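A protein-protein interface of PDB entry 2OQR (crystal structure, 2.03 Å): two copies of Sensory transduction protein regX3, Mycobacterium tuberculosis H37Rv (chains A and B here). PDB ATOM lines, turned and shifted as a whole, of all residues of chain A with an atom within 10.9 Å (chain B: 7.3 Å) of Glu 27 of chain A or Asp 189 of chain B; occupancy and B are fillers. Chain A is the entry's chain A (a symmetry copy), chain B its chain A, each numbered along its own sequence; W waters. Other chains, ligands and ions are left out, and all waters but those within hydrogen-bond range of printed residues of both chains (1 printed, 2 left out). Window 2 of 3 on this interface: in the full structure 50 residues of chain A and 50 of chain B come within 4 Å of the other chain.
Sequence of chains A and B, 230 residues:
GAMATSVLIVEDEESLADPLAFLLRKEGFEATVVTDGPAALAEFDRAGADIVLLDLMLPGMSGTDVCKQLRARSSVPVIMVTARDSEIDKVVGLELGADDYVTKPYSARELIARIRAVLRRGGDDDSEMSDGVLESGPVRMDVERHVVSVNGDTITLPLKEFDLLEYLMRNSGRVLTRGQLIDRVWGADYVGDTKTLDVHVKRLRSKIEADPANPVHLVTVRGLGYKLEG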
ATOM      1  N   ALA A   4      10.116  18.262   8.090  1.00  0.00           N
ATOM      2  CA  ALA A   4      10.579  18.864   6.803  1.00  0.00           C
ATOM      3  C   ALA A   4      10.782  20.358   7.021  1.00  0.00           C
ATOM      4  O   ALA A   4      10.235  20.923   7.996  1.00  0.00           O
ATOM      5  CB  ALA A   4       9.537  18.647   5.686  1.00  0.00           C
ATOM      6  N   THR A   5      11.521  20.985   6.104  1.00  0.00           N
ATOM      7  CA  THR A   5      11.772  22.433   6.125  1.00  0.00           C
ATOM      8  C   THR A   5      10.450  23.217   6.089  1.00  0.00           C
ATOM      9  O   THR A   5       9.561  22.916   5.295  1.00  0.00           O
ATOM     10  CB  THR A   5      12.708  22.844   4.956  1.00  0.00           C
ATOM     11  OG1 THR A   5      14.018  22.327   5.198  1.00  0.00           O
ATOM     12  CG2 THR A   5      12.791  24.373   4.800  1.00  0.00           C
ATOM     13  N   SER A   6      10.333  24.202   6.979  1.00  0.00           N
ATOM     14  CA  SER A   6       9.149  25.035   7.079  1.00  0.00           C
ATOM     15  C   SER A   6       9.366  26.419   6.440  1.00  0.00           C
ATOM     16  O   SER A   6      10.340  27.102   6.736  1.00  0.00           O
ATOM     17  CB  SER A   6       8.751  25.184   8.551  1.00  0.00           C
ATOM     18  OG  SER A   6       7.579  25.991   8.696  1.00  0.00           O
ATOM     19  N   VAL A   7       8.436  26.825   5.571  1.00  0.00           N
ATOM     20  CA  VAL A   7       8.503  28.121   4.896  1.00  0.00           C
ATOM     21  C   VAL A   7       7.301  28.934   5.357  1.00  0.00           C
ATOM     22  O   VAL A   7       6.180  28.470   5.254  1.00  0.00           O
ATOM     23  CB  VAL A   7       8.522  27.968   3.355  1.00  0.00           C
ATOM     24  CG1 VAL A   7       8.697  29.294   2.700  1.00  0.00           C
ATOM     25  CG2 VAL A   7       9.652  27.003   2.931  1.00  0.00           C
ATOM     26  N   PRO A  19      -0.101  29.862  -5.015  1.00  0.00           N
ATOM     27  CA  PRO A  19       0.642  28.977  -5.948  1.00  0.00           C
ATOM     28  C   PRO A  19       2.034  28.582  -5.496  1.00  0.00           C
ATOM     29  O   PRO A  19       2.494  27.481  -5.790  1.00  0.00           O
ATOM     30  CB  PRO A  19       0.761  29.819  -7.228  1.00  0.00           C
ATOM     31  CG  PRO A  19      -0.244  30.835  -7.130  1.00  0.00           C
ATOM     32  CD  PRO A  19      -0.474  31.122  -5.660  1.00  0.00           C
ATOM     33  N   LEU A  20       2.710  29.473  -4.785  1.00  0.00           N
ATOM     34  CA  LEU A  20       4.005  29.145  -4.228  1.00  0.00           C
ATOM     35  C   LEU A  20       3.833  28.121  -3.129  1.00  0.00           C
ATOM     36  O   LEU A  20       4.585  27.167  -3.066  1.00  0.00           O
ATOM     37  CB  LEU A  20       4.686  30.399  -3.672  1.00  0.00           C
ATOM     38  CG  LEU A  20       6.016  30.246  -2.936  1.00  0.00           C
ATOM     39  CD1 LEU A  20       7.017  29.432  -3.773  1.00  0.00           C
ATOM     40  CD2 LEU A  20       6.528  31.668  -2.596  1.00  0.00           C
ATOM     41  N   ALA A  21       2.851  28.341  -2.256  1.00  0.00           N
ATOM     42  CA  ALA A  21       2.563  27.424  -1.180  1.00  0.00           C
ATOM     43  C   ALA A  21       2.228  26.035  -1.741  1.00  0.00           C
ATOM     44  O   ALA A  21       2.703  25.019  -1.243  1.00  0.00           O
ATOM     45  CB  ALA A  21       1.413  27.959  -0.345  1.00  0.00           C
ATOM     46  N   PHE A  22       1.392  25.998  -2.767  1.00  0.00           N
ATOM     47  CA  PHE A  22       1.095  24.746  -3.462  1.00  0.00           C
ATOM     48  C   PHE A  22       2.359  23.993  -3.915  1.00  0.00           C
ATOM     49  O   PHE A  22       2.536  22.800  -3.618  1.00  0.00           O
ATOM     50  CB  PHE A  22       0.203  25.029  -4.670  1.00  0.00           C
ATOM     51  CG  PHE A  22      -0.233  23.798  -5.374  1.00  0.00           C
ATOM     52  CD1 PHE A  22      -1.299  23.047  -4.891  1.00  0.00           C
ATOM     53  CD2 PHE A  22       0.464  23.338  -6.491  1.00  0.00           C
ATOM     54  CE1 PHE A  22      -1.682  21.885  -5.524  1.00  0.00           C
ATOM     55  CE2 PHE A  22       0.069  22.170  -7.130  1.00  0.00           C
ATOM     56  CZ  PHE A  22      -0.998  21.450  -6.649  1.00  0.00           C
ATOM     57  N   LEU A  23       3.248  24.696  -4.600  1.00  0.00           N
ATOM     58  CA  LEU A  23       4.460  24.071  -5.165  1.00  0.00           C
ATOM     59  C   LEU A  23       5.395  23.584  -4.089  1.00  0.00           C
ATOM     60  O   LEU A  23       5.917  22.483  -4.164  1.00  0.00           O
ATOM     61  CB  LEU A  23       5.227  25.061  -6.017  1.00  0.00           C
ATOM     62  CG  LEU A  23       5.146  25.063  -7.525  1.00  0.00           C
ATOM     63  CD1 LEU A  23       6.410  25.774  -7.985  1.00  0.00           C
ATOM     64  CD2 LEU A  23       5.056  23.687  -8.143  1.00  0.00           C
ATOM     65  N   LEU A  24       5.642  24.433  -3.097  1.00  0.00           N
ATOM     66  CA  LEU A  24       6.409  24.020  -1.932  1.00  0.00           C
ATOM     67  C   LEU A  24       5.910  22.725  -1.324  1.00  0.00           C
ATOM     68  O   LEU A  24       6.696  21.836  -1.000  1.00  0.00           O
ATOM     69  CB  LEU A  24       6.378  25.101  -0.863  1.00  0.00           C
ATOM     70  CG  LEU A  24       7.302  26.248  -1.204  1.00  0.00           C
ATOM     71  CD1 LEU A  24       7.018  27.424  -0.303  1.00  0.00           C
ATOM     72  CD2 LEU A  24       8.811  25.850  -1.143  1.00  0.00           C
ATOM     73  N   ARG A  25       4.600  22.635  -1.140  1.00  0.00           N
ATOM     74  CA  ARG A  25       4.020  21.470  -0.497  1.00  0.00           C
ATOM     75  C   ARG A  25       4.213  20.252  -1.359  1.00  0.00           C
ATOM     76  O   ARG A  25       4.557  19.191  -0.850  1.00  0.00           O
ATOM     77  CB  ARG A  25       2.528  21.690  -0.225  1.00  0.00           C
ATOM     78  CG  ARG A  25       2.259  22.572   0.984  1.00  0.00           C
ATOM     79  CD  ARG A  25       0.761  22.965   1.092  1.00  0.00           C
ATOM     80  NE  ARG A  25       0.589  24.018   2.099  1.00  0.00           N
ATOM     81  CZ  ARG A  25      -0.192  25.079   1.970  1.00  0.00           C
ATOM     82  NH1 ARG A  25      -0.915  25.269   0.876  1.00  0.00           N
ATOM     83  NH2 ARG A  25      -0.234  25.980   2.946  1.00  0.00           N
ATOM     84  N   LYS A  26       4.019  20.387  -2.666  1.00  0.00           N
ATOM     85  CA  LYS A  26       4.181  19.221  -3.562  1.00  0.00           C
ATOM     86  C   LYS A  26       5.663  18.769  -3.660  1.00  0.00           C
ATOM     87  O   LYS A  26       5.952  17.660  -4.121  1.00  0.00           O
ATOM     88  CB  LYS A  26       3.542  19.500  -4.947  1.00  0.00           C
ATOM     89  CG  LYS A  26       4.462  19.776  -6.118  1.00  0.00           C
ATOM     90  CD  LYS A  26       4.448  18.636  -7.169  1.00  0.00           C
ATOM     91  CE  LYS A  26       5.628  18.711  -8.184  1.00  0.00           C
ATOM     92  NZ  LYS A  26       5.955  20.095  -8.725  1.00  0.00           N
ATOM     93  N   GLU A  27       6.582  19.643  -3.237  1.00  0.00           N
ATOM     94  CA  GLU A  27       8.025  19.360  -3.241  1.00  0.00           C
ATOM     95  C   GLU A  27       8.545  18.950  -1.856  1.00  0.00           C
ATOM     96  O   GLU A  27       9.737  18.727  -1.686  1.00  0.00           O
ATOM     97  CB  GLU A  27       8.812  20.549  -3.821  1.00  0.00           C
ATOM     98  CG  GLU A  27       8.630  20.773  -5.344  1.00  0.00           C
ATOM     99  CD  GLU A  27       9.081  19.588  -6.206  1.00  0.00           C
ATOM    100  OE1 GLU A  27       9.842  18.724  -5.721  1.00  0.00           O
ATOM    101  OE2 GLU A  27       8.644  19.464  -7.372  1.00  0.00           O
ATOM    102  N   GLY A  28       7.637  18.769  -0.892  1.00  0.00           N
ATOM    103  CA  GLY A  28       7.987  18.183   0.414  1.00  0.00           C
ATOM    104  C   GLY A  28       8.313  19.167   1.530  1.00  0.00           C
ATOM    105  O   GLY A  28       8.809  18.775   2.610  1.00  0.00           O
ATOM    106  N   PHE A  29       8.067  20.449   1.273  1.00  0.00           N
ATOM    107  CA  PHE A  29       8.221  21.499   2.289  1.00  0.00           C
ATOM    108  C   PHE A  29       6.906  21.748   3.015  1.00  0.00           C
ATOM    109  O   PHE A  29       5.861  21.518   2.446  1.00  0.00           O
ATOM    110  CB  PHE A  29       8.575  22.812   1.621  1.00  0.00           C
ATOM    111  CG  PHE A  29       9.904  22.819   0.920  1.00  0.00           C
ATOM    112  CD1 PHE A  29      11.025  23.271   1.563  1.00  0.00           C
ATOM    113  CD2 PHE A  29      10.009  22.389  -0.404  1.00  0.00           C
ATOM    114  CE1 PHE A  29      12.254  23.302   0.897  1.00  0.00           C
ATOM    115  CE2 PHE A  29      11.206  22.422  -1.075  1.00  0.00           C
ATOM    116  CZ  PHE A  29      12.337  22.880  -0.439  1.00  0.00           C
ATOM    117  N   GLU A  30       6.954  22.274   4.244  1.00  0.00           N
ATOM    118  CA  GLU A  30       5.744  22.792   4.872  1.00  0.00           C
ATOM    119  C   GLU A  30       5.680  24.236   4.453  1.00  0.00           C
ATOM    120  O   GLU A  30       6.714  24.888   4.347  1.00  0.00           O
ATOM    121  CB  GLU A  30       5.786  22.750   6.394  1.00  0.00           C
ATOM    122  CG  GLU A  30       6.369  21.515   7.006  1.00  0.00           C
ATOM    123  CD  GLU A  30       6.374  21.606   8.544  1.00  0.00           C
ATOM    124  OE1 GLU A  30       7.298  20.995   9.170  1.00  0.00           O
ATOM    125  OE2 GLU A  30       5.470  22.313   9.101  1.00  0.00           O
ATOM    126  N   ALA A  31       4.482  24.731   4.173  1.00  0.00           N
ATOM    127  CA  ALA A  31       4.295  26.155   3.843  1.00  0.00           C
ATOM    128  C   ALA A  31       3.099  26.678   4.642  1.00  0.00           C
ATOM    129  O   ALA A  31       2.126  25.970   4.775  1.00  0.00           O
ATOM    130  CB  ALA A  31       4.099  26.351   2.350  1.00  0.00           C
ATOM    131  N   ARG B 109       9.193  28.523  -8.911  1.00  0.00           N
ATOM    132  CA  ARG B 109      10.108  27.400  -9.025  1.00  0.00           C
ATOM    133  C   ARG B 109      11.544  27.836  -8.821  1.00  0.00           C
ATOM    134  O   ARG B 109      12.341  27.150  -8.203  1.00  0.00           O
ATOM    135  CB  ARG B 109       9.945  26.721 -10.387  1.00  0.00           C
ATOM    136  CG  ARG B 109       8.800  25.729 -10.398  1.00  0.00           C
ATOM    137  CD  ARG B 109       8.356  25.423 -11.811  1.00  0.00           C
ATOM    138  NE  ARG B 109       7.238  24.486 -11.816  1.00  0.00           N
ATOM    139  CZ  ARG B 109       5.974  24.851 -11.929  1.00  0.00           C
ATOM    140  NH1 ARG B 109       5.013  23.938 -11.937  1.00  0.00           N
ATOM    141  NH2 ARG B 109       5.670  26.129 -12.007  1.00  0.00           N
ATOM    142  N   ILE B 112      12.077  28.272  -5.246  1.00  0.00           N
ATOM    143  CA  ILE B 112      12.325  26.942  -4.644  1.00  0.00           C
ATOM    144  C   ILE B 112      13.740  26.436  -4.893  1.00  0.00           C
ATOM    145  O   ILE B 112      14.390  25.895  -3.995  1.00  0.00           O
ATOM    146  CB  ILE B 112      11.279  25.919  -5.099  1.00  0.00           C
ATOM    147  CG1 ILE B 112       9.884  26.364  -4.640  1.00  0.00           C
ATOM    148  CG2 ILE B 112      11.582  24.593  -4.480  1.00  0.00           C
ATOM    149  CD1 ILE B 112       8.789  25.405  -5.107  1.00  0.00           C
ATOM    150  N   ARG B 116      16.432  25.387  -1.969  1.00  0.00           N
ATOM    151  CA  ARG B 116      17.184  24.112  -1.889  1.00  0.00           C
ATOM    152  C   ARG B 116      18.675  24.338  -1.823  1.00  0.00           C
ATOM    153  O   ARG B 116      19.405  23.663  -1.089  1.00  0.00           O
ATOM    154  CB  ARG B 116      16.889  23.174  -3.091  1.00  0.00           C
ATOM    155  CG  ARG B 116      15.455  22.796  -3.311  1.00  0.00           C
ATOM    156  CD  ARG B 116      15.353  22.063  -4.636  1.00  0.00           C
ATOM    157  NE  ARG B 116      14.001  21.730  -5.033  1.00  0.00           N
ATOM    158  CZ  ARG B 116      13.313  20.650  -4.672  1.00  0.00           C
ATOM    159  NH1 ARG B 116      13.787  19.742  -3.856  1.00  0.00           N
ATOM    160  NH2 ARG B 116      12.128  20.476  -5.135  1.00  0.00           N
ATOM    161  N   ARG B 178      15.872  12.352 -14.044  1.00  0.00           N
ATOM    162  CA  ARG B 178      15.285  13.566 -14.548  1.00  0.00           C
ATOM    163  C   ARG B 178      14.639  14.354 -13.405  1.00  0.00           C
ATOM    164  O   ARG B 178      14.821  15.564 -13.329  1.00  0.00           O
ATOM    165  CB  ARG B 178      14.287  13.296 -15.711  1.00  0.00           C
ATOM    166  CG  ARG B 178      13.042  12.541 -15.325  1.00  0.00           C
ATOM    167  CD  ARG B 178      12.372  11.814 -16.541  1.00  0.00           C
ATOM    168  NE  ARG B 178      11.345  10.885 -16.082  1.00  0.00           N
ATOM    169  CZ  ARG B 178      10.106  11.226 -15.734  1.00  0.00           C
ATOM    170  NH1 ARG B 178       9.687  12.470 -15.835  1.00  0.00           N
ATOM    171  NH2 ARG B 178       9.264  10.298 -15.329  1.00  0.00           N
ATOM    172  N   GLY B 179      13.915  13.671 -12.522  1.00  0.00           N
ATOM    173  CA  GLY B 179      13.302  14.311 -11.368  1.00  0.00           C
ATOM    174  C   GLY B 179      14.292  14.967 -10.417  1.00  0.00           C
ATOM    175  O   GLY B 179      14.052  16.074  -9.904  1.00  0.00           O
ATOM    176  N   GLN B 180      15.395  14.295 -10.135  1.00  0.00           N
ATOM    177  CA  GLN B 180      16.429  14.882  -9.286  1.00  0.00           C
ATOM    178  C   GLN B 180      16.999  16.091  -9.956  1.00  0.00           C
ATOM    179  O   GLN B 180      17.182  17.136  -9.318  1.00  0.00           O
ATOM    180  CB  GLN B 180      17.570  13.894  -9.010  1.00  0.00           C
ATOM    181  CG  GLN B 180      17.221  12.817  -8.060  1.00  0.00           C
ATOM    182  CD  GLN B 180      18.285  11.766  -7.994  1.00  0.00           C
ATOM    183  OE1 GLN B 180      18.714  11.246  -9.012  1.00  0.00           O
ATOM    184  NE2 GLN B 180      18.734  11.460  -6.787  1.00  0.00           N
ATOM    185  N   ILE B 182      15.777  17.961 -12.394  1.00  0.00           N
ATOM    186  CA  ILE B 182      14.837  19.060 -12.540  1.00  0.00           C
ATOM    187  C   ILE B 182      14.616  19.824 -11.218  1.00  0.00           C
ATOM    188  O   ILE B 182      14.661  21.065 -11.196  1.00  0.00           O
ATOM    189  CB  ILE B 182      13.537  18.553 -13.139  1.00  0.00           C
ATOM    190  CG1 ILE B 182      13.765  18.280 -14.636  1.00  0.00           C
ATOM    191  CG2 ILE B 182      12.391  19.575 -12.926  1.00  0.00           C
ATOM    192  CD1 ILE B 182      12.759  17.268 -15.262  1.00  0.00           C
ATOM    193  N   ASP B 183      14.386  19.094 -10.122  1.00  0.00           N
ATOM    194  CA  ASP B 183      14.213  19.710  -8.798  1.00  0.00           C
ATOM    195  C   ASP B 183      15.399  20.594  -8.423  1.00  0.00           C
ATOM    196  O   ASP B 183      15.240  21.704  -7.917  1.00  0.00           O
ATOM    197  CB  ASP B 183      13.991  18.644  -7.695  1.00  0.00           C
ATOM    198  CG  ASP B 183      12.560  18.123  -7.664  1.00  0.00           C
ATOM    199  OD1 ASP B 183      11.693  18.750  -8.303  1.00  0.00           O
ATOM    200  OD2 ASP B 183      12.304  17.091  -6.974  1.00  0.00           O
ATOM    201  N   TRP B 186      16.013  23.524 -11.736  1.00  0.00           N
ATOM    202  CA  TRP B 186      14.854  24.379 -12.010  1.00  0.00           C
ATOM    203  C   TRP B 186      13.913  24.555 -10.816  1.00  0.00           C
ATOM    204  O   TRP B 186      13.051  25.433 -10.826  1.00  0.00           O
ATOM    205  CB  TRP B 186      14.077  23.839 -13.193  1.00  0.00           C
ATOM    206  CG  TRP B 186      14.750  24.126 -14.465  1.00  0.00           C
ATOM    207  CD1 TRP B 186      14.665  25.280 -15.209  1.00  0.00           C
ATOM    208  CD2 TRP B 186      15.672  23.286 -15.136  1.00  0.00           C
ATOM    209  NE1 TRP B 186      15.461  25.184 -16.319  1.00  0.00           N
ATOM    210  CE2 TRP B 186      16.095  23.971 -16.301  1.00  0.00           C
ATOM    211  CE3 TRP B 186      16.178  22.011 -14.881  1.00  0.00           C
ATOM    212  CZ2 TRP B 186      17.004  23.426 -17.194  1.00  0.00           C
ATOM    213  CZ3 TRP B 186      17.094  21.462 -15.785  1.00  0.00           C
ATOM    214  CH2 TRP B 186      17.492  22.169 -16.921  1.00  0.00           C
ATOM    215  N   GLY B 187      14.087  23.746  -9.778  1.00  0.00           N
ATOM    216  CA  GLY B 187      13.416  23.965  -8.516  1.00  0.00           C
ATOM    217  C   GLY B 187      12.269  23.034  -8.206  1.00  0.00           C
ATOM    218  O   GLY B 187      12.082  22.657  -7.074  1.00  0.00           O
ATOM    219  N   ALA B 188      11.456  22.737  -9.215  1.00  0.00           N
ATOM    220  CA  ALA B 188      10.260  21.924  -9.058  1.00  0.00           C
ATOM    221  C   ALA B 188       9.883  21.464 -10.448  1.00  0.00           C
ATOM    222  O   ALA B 188      10.322  22.066 -11.446  1.00  0.00           O
ATOM    223  CB  ALA B 188       9.136  22.740  -8.420  1.00  0.00           C
ATOM    224  N   ASP B 189       9.096  20.390 -10.525  1.00  0.00           N
ATOM    225  CA  ASP B 189       8.674  19.842 -11.805  1.00  0.00           C
ATOM    226  C   ASP B 189       7.712  20.796 -12.483  1.00  0.00           C
ATOM    227  O   ASP B 189       7.011  21.557 -11.804  1.00  0.00           O
ATOM    228  CB  ASP B 189       8.064  18.449 -11.608  1.00  0.00           C
ATOM    229  CG  ASP B 189       8.999  17.542 -10.831  1.00  0.00           C
ATOM    230  OD1 ASP B 189       9.841  16.861 -11.474  1.00  0.00           O
ATOM    231  OD2 ASP B 189       8.954  17.579  -9.561  1.00  0.00           O
ATOM    232  N   TYR B 190       7.722  20.814 -13.817  1.00  0.00           N
ATOM    233  CA  TYR B 190       6.854  21.716 -14.576  1.00  0.00           C
ATOM    234  C   TYR B 190       6.600  21.191 -15.968  1.00  0.00           C
ATOM    235  O   TYR B 190       7.331  20.351 -16.450  1.00  0.00           O
ATOM    236  CB  TYR B 190       7.454  23.122 -14.643  1.00  0.00           C
ATOM    237  CG  TYR B 190       8.784  23.219 -15.373  1.00  0.00           C
ATOM    238  CD1 TYR B 190       8.835  23.574 -16.706  1.00  0.00           C
ATOM    239  CD2 TYR B 190       9.986  22.963 -14.720  1.00  0.00           C
ATOM    240  CE1 TYR B 190      10.050  23.678 -17.384  1.00  0.00           C
ATOM    241  CE2 TYR B 190      11.212  23.052 -15.394  1.00  0.00           C
ATOM    242  CZ  TYR B 190      11.228  23.418 -16.727  1.00  0.00           C
ATOM    243  OH  TYR B 190      12.410  23.522 -17.426  1.00  0.00           O
ATOM    244  N   VAL B 191       5.551  21.693 -16.602  1.00  0.00           N
ATOM    245  CA  VAL B 191       5.187  21.264 -17.951  1.00  0.00           C
ATOM    246  C   VAL B 191       6.349  21.542 -18.919  1.00  0.00           C
ATOM    247  O   VAL B 191       6.837  22.660 -19.006  1.00  0.00           O
ATOM    248  CB  VAL B 191       3.873  21.906 -18.403  1.00  0.00           C
ATOM    249  CG1 VAL B 191       3.578  21.580 -19.869  1.00  0.00           C
ATOM    250  CG2 VAL B 191       2.725  21.416 -17.503  1.00  0.00           C
ATOM    251  N   GLY B 192       6.808  20.499 -19.614  1.00  0.00           N
ATOM    252  CA  GLY B 192       7.905  20.632 -20.565  1.00  0.00           C
ATOM    253  C   GLY B 192       9.290  20.515 -19.949  1.00  0.00           C
ATOM    254  O   GLY B 192      10.272  20.754 -20.621  1.00  0.00           O
ATOM    255  N   ASP B 193       9.379  20.111 -18.689  1.00  0.00           N
ATOM    256  CA  ASP B 193      10.677  20.023 -18.008  1.00  0.00           C
ATOM    257  C   ASP B 193      11.645  18.997 -18.565  1.00  0.00           C
ATOM    258  O   ASP B 193      12.819  19.271 -18.652  1.00  0.00           O
ATOM    259  CB  ASP B 193      10.540  19.883 -16.476  1.00  0.00           C
ATOM    260  CG  ASP B 193       9.617  18.745 -16.023  1.00  0.00           C
ATOM    261  OD1 ASP B 193       9.136  17.923 -16.842  1.00  0.00           O
ATOM    262  OD2 ASP B 193       9.351  18.701 -14.797  1.00  0.00           O
HETATM  263  O   HOH W   1      11.568  17.816  -3.433  1.00  0.00           O
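The side-chain carboxylate (OE1) of Glu 27 of chain A lies close to the guanidinium group (NH2) of Arg 116 of chain B, 2.9 Å away.
The side-chain carboxylate (OD1) of Asp 183 of chain B lies close to the side-chain carboxylate (OE1) of Glu 27 of chain A.
The side-chain carboxylate of Asp 189 of chain B lies close to the side-chain carboxylate of Glu 27 of chain A (2.9 Å).
Of the printed residues of chain B, Leu 23 of chain A touches Arg 109 (3.4 Å) and Ile 112 (3.7 Å).
Of the printed residues of chain B, Lys 26 of chain A touches Asp 189.
Glu 27 of chain A touches just these residues of chain B: Arg 116, Asp 183, Ala 188 and Asp 189.
Of the printed residues of chain A, Ile 112 of chain B touches Leu 23 (3.7 Å) and Leu 24 (3.7 Å).
Printed residues of chain A within 4 Å of Arg 116 of chain B: Glu 27 (2.9 Å).
Asp 183 of chain B touches one residue of chain A.
No residue of chain A comes within 4 Å of Gly 187 of chain B.
Of the printed residues of chain A, Ala 188 of chain B touches Glu 27.
Asp 189 of chain B touches just these residues of chain A: Lys 26 and Glu 27.
The nearest residue of chain B that does not touch Glu 27 of chain A is Gly 187 of chain B (4.3 Å).
The nearest residue of chain A that does not touch Asp 189 of chain B is Leu 23 of chain A (4.7 Å).
CG of Arg 109 of chain B touches CD1 of Leu 23 of chain A (3.4 Å).
Ile 112 of chain B touches Leu 23 of chain A.
CD2 of Leu 24 of chain A touches CG1 of Ile 112 of chain B, at 3.7 Å.
Lys 26 of chain A touches Asp 189 of chain B (NZ to O, 3.6 Å).
CA of Ala 188 of chain B touches OE2 of Glu 27 of chain A (3.4 Å).
Water W1 bridges O of Glu 27 of chain A and NH1 of Arg 116 of chain B.
Printed residues of chain A that touch a printed residue of chain B: Leu 23, Leu 24, Lys 26 and Glu 27.
Of the 16 printed residues of chain B, 6 touch a printed residue of chain A.
Hydrophobic or aromatic side chains of chain B within 4 Å of the printed part of chain A: Ile 112 and Ala 188.
Along chain B the printed residues that touch a printed residue of chain A span positions 109 to 189.
Among the printed residues, 8 pairs touch across the chains.
The backbone carbonyl oxygen (O) of Asp 189 of chain B is in hydrogen-bond range of the guanidinium group (NE) of Arg 109 of chain B (2.9 Å).
The guanidinium group (NE) of Arg 116 of chain B is in hydrogen-bond range of the backbone carbonyl oxygen (O) of Asp 183 of chain B, at 3.1 Å.
O of Gly 187 of chain B lies within hydrogen-bond range of NH2 of Arg 116 of chain B (2.9 Å).
O of Leu 24 of chain A is in hydrogen-bond range of N of Phe 29 of chain A.
The side-chain amino group (NZ) of Lys 26 of chain A is in salt-bridge range of the side-chain carboxylate (OE2) of Glu 27 of chain A (3.1 Å).
No position is printed for both chains.
Of the 8 pairs that touch across the chains among the printed residues, none has its exchanged pair printed and touching as well.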
